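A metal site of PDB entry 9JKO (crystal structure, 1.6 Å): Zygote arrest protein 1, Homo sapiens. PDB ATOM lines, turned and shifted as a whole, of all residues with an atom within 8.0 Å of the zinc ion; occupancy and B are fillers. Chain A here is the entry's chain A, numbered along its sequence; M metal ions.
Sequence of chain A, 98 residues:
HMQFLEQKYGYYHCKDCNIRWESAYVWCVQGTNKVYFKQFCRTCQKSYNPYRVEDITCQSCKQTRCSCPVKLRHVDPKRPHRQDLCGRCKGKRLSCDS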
ATOM      1  N   HIS A  13      -4.523   3.044   5.232  1.00  0.00           N
ATOM      2  CA  HIS A  13      -3.448   2.956   4.250  1.00  0.00           C
ATOM      3  C   HIS A  13      -3.617   1.682   3.443  1.00  0.00           C
ATOM      4  O   HIS A  13      -3.504   0.592   3.996  1.00  0.00           O
ATOM      5  CB  HIS A  13      -2.092   3.010   4.964  1.00  0.00           C
ATOM      6  CG  HIS A  13      -0.903   3.031   4.039  1.00  0.00           C
ATOM      7  ND1 HIS A  13       0.318   2.513   4.405  1.00  0.00           N
ATOM      8  CD2 HIS A  13      -0.771   3.445   2.757  1.00  0.00           C
ATOM      9  CE1 HIS A  13       1.169   2.665   3.400  1.00  0.00           C
ATOM     10  NE2 HIS A  13       0.540   3.232   2.391  1.00  0.00           N
ATOM     11  N   CYS A  14      -3.867   1.817   2.140  1.00  0.00           N
ATOM     12  CA  CYS A  14      -3.779   0.664   1.245  1.00  0.00           C
ATOM     13  C   CYS A  14      -2.339   0.579   0.752  1.00  0.00           C
ATOM     14  O   CYS A  14      -1.883   1.432  -0.007  1.00  0.00           O
ATOM     15  CB  CYS A  14      -4.760   0.804   0.073  1.00  0.00           C
ATOM     16  SG  CYS A  14      -4.442  -0.443  -1.240  1.00  0.00           S
ATOM     17  N   LYS A  15      -1.602  -0.413   1.207  1.00  0.00           N
ATOM     18  CA  LYS A  15      -0.180  -0.526   0.827  1.00  0.00           C
ATOM     19  C   LYS A  15      -0.046  -0.968  -0.634  1.00  0.00           C
ATOM     20  O   LYS A  15       0.953  -0.615  -1.259  1.00  0.00           O
ATOM     21  CB  LYS A  15       0.473  -1.586   1.719  1.00  0.00           C
ATOM     22  CG  LYS A  15       0.816  -1.077   3.105  1.00  0.00           C
ATOM     23  CD  LYS A  15       0.756  -2.197   4.131  1.00  0.00           C
ATOM     24  CE  LYS A  15       1.079  -1.715   5.499  1.00  0.00           C
ATOM     25  NZ  LYS A  15      -0.151  -1.245   6.157  1.00  0.00           N
ATOM     26  N   ASP A  16      -1.013  -1.746  -1.128  1.00  0.00           N
ATOM     27  CA  ASP A  16      -0.929  -2.189  -2.519  1.00  0.00           C
ATOM     28  C   ASP A  16      -0.953  -1.011  -3.500  1.00  0.00           C
ATOM     29  O   ASP A  16      -0.193  -1.024  -4.477  1.00  0.00           O
ATOM     30  CB  ASP A  16      -2.053  -3.171  -2.844  1.00  0.00           C
ATOM     31  CG  ASP A  16      -2.064  -4.371  -1.920  1.00  0.00           C
ATOM     32  OD1 ASP A  16      -0.952  -4.857  -1.565  1.00  0.00           O
ATOM     33  OD2 ASP A  16      -3.150  -4.918  -1.633  1.00  0.00           O
ATOM     34  N   CYS A  17      -1.786  -0.017  -3.259  1.00  0.00           N
ATOM     35  CA  CYS A  17      -1.860   1.170  -4.119  1.00  0.00           C
ATOM     36  C   CYS A  17      -1.055   2.338  -3.583  1.00  0.00           C
ATOM     37  O   CYS A  17      -0.939   3.352  -4.278  1.00  0.00           O
ATOM     38  CB  CYS A  17      -3.325   1.614  -4.317  1.00  0.00           C
ATOM     39  SG  CYS A  17      -4.422   0.302  -4.873  1.00  0.00           S
ATOM     40  N   ASN A  18      -0.529   2.209  -2.366  1.00  0.00           N
ATOM     41  CA  ASN A  18       0.080   3.302  -1.618  1.00  0.00           C
ATOM     42  C   ASN A  18      -0.806   4.555  -1.622  1.00  0.00           C
ATOM     43  O   ASN A  18      -0.430   5.646  -2.042  1.00  0.00           O
ATOM     44  CB  ASN A  18       1.506   3.598  -2.092  1.00  0.00           C
ATOM     45  CG  ASN A  18       2.143   4.695  -1.247  1.00  0.00           C
ATOM     46  OD1 ASN A  18       2.016   4.648  -0.011  1.00  0.00           O
ATOM     47  ND2 ASN A  18       2.938   5.579  -1.877  1.00  0.00           N
ATOM     48  N   ILE A  19      -1.998   4.364  -1.049  1.00  0.00           N
ATOM     49  CA  ILE A  19      -2.990   5.412  -0.892  1.00  0.00           C
ATOM     50  C   ILE A  19      -3.350   5.492   0.580  1.00  0.00           C
ATOM     51  O   ILE A  19      -3.730   4.482   1.187  1.00  0.00           O
ATOM     52  CB  ILE A  19      -4.245   5.135  -1.723  1.00  0.00           C
ATOM     53  CG1 ILE A  19      -3.922   5.338  -3.207  1.00  0.00           C
ATOM     54  CG2 ILE A  19      -5.378   6.097  -1.323  1.00  0.00           C
ATOM     55  CD1 ILE A  19      -4.977   4.807  -4.081  1.00  0.00           C
ATOM     56  N   TRP A  21      -5.825   7.440   3.443  1.00  0.00           N
ATOM     57  CA  TRP A  21      -6.985   8.298   3.568  1.00  0.00           C
ATOM     58  C   TRP A  21      -7.410   8.330   5.029  1.00  0.00           C
ATOM     59  O   TRP A  21      -6.958   7.526   5.833  1.00  0.00           O
ATOM     60  CB  TRP A  21      -8.151   7.861   2.666  1.00  0.00           C
ATOM     61  CG  TRP A  21      -8.904   6.623   3.050  1.00  0.00           C
ATOM     62  CD1 TRP A  21     -10.060   6.545   3.815  1.00  0.00           C
ATOM     63  CD2 TRP A  21      -8.609   5.301   2.651  1.00  0.00           C
ATOM     64  NE1 TRP A  21     -10.485   5.263   3.880  1.00  0.00           N
ATOM     65  CE2 TRP A  21      -9.608   4.469   3.175  1.00  0.00           C
ATOM     66  CE3 TRP A  21      -7.599   4.735   1.853  1.00  0.00           C
ATOM     67  CZ2 TRP A  21      -9.598   3.090   2.993  1.00  0.00           C
ATOM     68  CZ3 TRP A  21      -7.593   3.388   1.672  1.00  0.00           C
ATOM     69  CH2 TRP A  21      -8.607   2.569   2.209  1.00  0.00           C
ATOM     70  N   PHE A  40     -13.390   1.306   1.519  1.00  0.00           N
ATOM     71  CA  PHE A  40     -12.826   0.723   0.317  1.00  0.00           C
ATOM     72  C   PHE A  40     -11.783   1.648  -0.302  1.00  0.00           C
ATOM     73  O   PHE A  40     -11.963   2.869  -0.321  1.00  0.00           O
ATOM     74  CB  PHE A  40     -13.981   0.396  -0.654  1.00  0.00           C
ATOM     75  CG  PHE A  40     -14.872  -0.683  -0.118  1.00  0.00           C
ATOM     76  CD1 PHE A  40     -14.579  -2.016  -0.396  1.00  0.00           C
ATOM     77  CD2 PHE A  40     -15.923  -0.374   0.747  1.00  0.00           C
ATOM     78  CE1 PHE A  40     -15.335  -3.051   0.160  1.00  0.00           C
ATOM     79  CE2 PHE A  40     -16.676  -1.400   1.303  1.00  0.00           C
ATOM     80  CZ  PHE A  40     -16.398  -2.740   1.007  1.00  0.00           C
ATOM     81  N   CYS A  41     -10.681   1.061  -0.781  1.00  0.00           N
ATOM     82  CA  CYS A  41      -9.649   1.857  -1.434  1.00  0.00           C
ATOM     83  C   CYS A  41     -10.174   2.395  -2.765  1.00  0.00           C
ATOM     84  O   CYS A  41     -10.754   1.643  -3.564  1.00  0.00           O
ATOM     85  CB  CYS A  41      -8.408   1.013  -1.643  1.00  0.00           C
ATOM     86  SG  CYS A  41      -7.130   1.803  -2.660  1.00  0.00           S
ATOM     87  N   ARG A  42      -9.954   3.679  -2.999  1.00  0.00           N
ATOM     88  CA  ARG A  42     -10.531   4.298  -4.187  1.00  0.00           C
ATOM     89  C   ARG A  42      -9.906   3.774  -5.468  1.00  0.00           C
ATOM     90  O   ARG A  42     -10.482   3.942  -6.543  1.00  0.00           O
ATOM     91  CB  ARG A  42     -10.377   5.817  -4.116  1.00  0.00           C
ATOM     92  CG  ARG A  42      -8.942   6.352  -4.227  1.00  0.00           C
ATOM     93  CD  ARG A  42      -8.952   7.876  -4.393  1.00  0.00           C
ATOM     94  NE  ARG A  42      -7.623   8.450  -4.201  1.00  0.00           N
ATOM     95  CZ  ARG A  42      -7.184   8.911  -3.036  1.00  0.00           C
ATOM     96  NH1 ARG A  42      -7.877   8.726  -1.917  1.00  0.00           N
ATOM     97  NH2 ARG A  42      -6.001   9.537  -2.970  1.00  0.00           N
ATOM     98  N   THR A  43      -8.766   3.091  -5.380  1.00  0.00           N
ATOM     99  CA  THR A  43      -8.124   2.604  -6.601  1.00  0.00           C
ATOM    100  C   THR A  43      -8.368   1.115  -6.808  1.00  0.00           C
ATOM    101  O   THR A  43      -8.917   0.716  -7.840  1.00  0.00           O
ATOM    102  CB  THR A  43      -6.636   2.933  -6.577  1.00  0.00           C
ATOM    103  OG1 THR A  43      -6.498   4.327  -6.875  1.00  0.00           O
ATOM    104  CG2 THR A  43      -5.939   2.159  -7.688  1.00  0.00           C
ATOM    105  N   CYS A  44      -8.030   0.261  -5.825  1.00  0.00           N
ATOM    106  CA  CYS A  44      -8.166  -1.179  -6.006  1.00  0.00           C
ATOM    107  C   CYS A  44      -9.502  -1.728  -5.547  1.00  0.00           C
ATOM    108  O   CYS A  44      -9.811  -2.897  -5.789  1.00  0.00           O
ATOM    109  CB  CYS A  44      -7.033  -1.927  -5.280  1.00  0.00           C
ATOM    110  SG  CYS A  44      -7.144  -1.922  -3.467  1.00  0.00           S
ATOM    111  N   GLN A  45     -10.293  -0.919  -4.845  1.00  0.00           N
ATOM    112  CA  GLN A  45     -11.631  -1.273  -4.387  1.00  0.00           C
ATOM    113  C   GLN A  45     -11.645  -2.474  -3.422  1.00  0.00           C
ATOM    114  O   GLN A  45     -12.704  -3.036  -3.141  1.00  0.00           O
ATOM    115  CB  GLN A  45     -12.550  -1.513  -5.596  1.00  0.00           C
ATOM    116  CG  GLN A  45     -12.753  -0.219  -6.369  1.00  0.00           C
ATOM    117  CD  GLN A  45     -13.859   0.644  -5.755  1.00  0.00           C
ATOM    118  OE1 GLN A  45     -14.452   0.265  -4.731  1.00  0.00           O
ATOM    119  NE2 GLN A  45     -14.089   1.829  -6.316  1.00  0.00           N
ATOM    120  N   LYS A  46     -10.518  -2.842  -2.811  1.00  0.00           N
ATOM    121  CA  LYS A  46     -10.607  -3.804  -1.722  1.00  0.00           C
ATOM    122  C   LYS A  46     -11.007  -3.102  -0.429  1.00  0.00           C
ATOM    123  O   LYS A  46     -10.907  -1.878  -0.322  1.00  0.00           O
ATOM    124  CB  LYS A  46      -9.272  -4.528  -1.475  1.00  0.00           C
ATOM    125  CG  LYS A  46      -8.793  -5.329  -2.673  1.00  0.00           C
ATOM    126  CD  LYS A  46      -7.583  -6.160  -2.359  1.00  0.00           C
ATOM    127  CE  LYS A  46      -6.515  -5.292  -1.747  1.00  0.00           C
ATOM    128  NZ  LYS A  46      -5.517  -4.956  -2.717  1.00  0.00           N
ATOM    129  N   SER A  47     -11.414  -3.906   0.556  1.00  0.00           N
ATOM    130  CA  SER A  47     -11.936  -3.444   1.848  1.00  0.00           C
ATOM    131  C   SER A  47     -10.819  -3.304   2.878  1.00  0.00           C
ATOM    132  O   SER A  47      -9.897  -4.115   2.936  1.00  0.00           O
ATOM    133  CB  SER A  47     -13.000  -4.406   2.387  1.00  0.00           C
ATOM    134  OG  SER A  47     -12.449  -5.684   2.698  1.00  0.00           O
ATOM    135  N   TYR A  48     -10.963  -2.303   3.746  1.00  0.00           N
ATOM    136  CA  TYR A  48      -9.939  -2.031   4.746  1.00  0.00           C
ATOM    137  C   TYR A  48     -10.537  -1.615   6.069  1.00  0.00           C
ATOM    138  O   TYR A  48     -11.549  -0.919   6.102  1.00  0.00           O
ATOM    139  CB  TYR A  48      -9.005  -0.901   4.276  1.00  0.00           C
ATOM    140  CG  TYR A  48      -8.069  -1.398   3.209  1.00  0.00           C
ATOM    141  CD1 TYR A  48      -6.871  -2.023   3.564  1.00  0.00           C
ATOM    142  CD2 TYR A  48      -8.380  -1.281   1.865  1.00  0.00           C
ATOM    143  CE1 TYR A  48      -6.017  -2.505   2.602  1.00  0.00           C
ATOM    144  CE2 TYR A  48      -7.508  -1.766   0.890  1.00  0.00           C
ATOM    145  CZ  TYR A  48      -6.345  -2.375   1.271  1.00  0.00           C
ATOM    146  OH  TYR A  48      -5.496  -2.855   0.280  1.00  0.00           O
HETATM  147 ZN    ZN M   1      -5.778  -0.031  -3.052  1.00  0.00          ZN
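SG of Cys 41 sits close to N of Thr 43, at 3.4 Å. The side-chain sulfur (SG) of Cys 14 lies close to the backbone NH (N) of Asp 16. The side-chain sulfur of Cys 44 lies close to the side-chain amino group of Lys 46 (3.5 Å). The backbone carbonyl oxygen (O) of Ile 19 sits at hydrogen-bond distance from the backbone NH (N) of Cys 14, 2.8 Å away. N of Cys 41 is in hydrogen-bond range of O of Lys 46, at 3.0 Å. The side-chain hydroxyl (OH) of Tyr 48 lies close to the side-chain sulfur (SG) of Cys 14, at 3.0 Å.
Of the 17 residues printed, 4 come within 4 Å of the zinc ion.
SG of Cys 14 is bound to the zinc ion, at 2.3 Å. SG of Cys 17 binds the zinc ion, at 2.3 Å. The zinc ion is bound by SG of Cys 41 (2.3 Å). SG of Cys 44 binds the zinc ion, at 2.4 Å.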
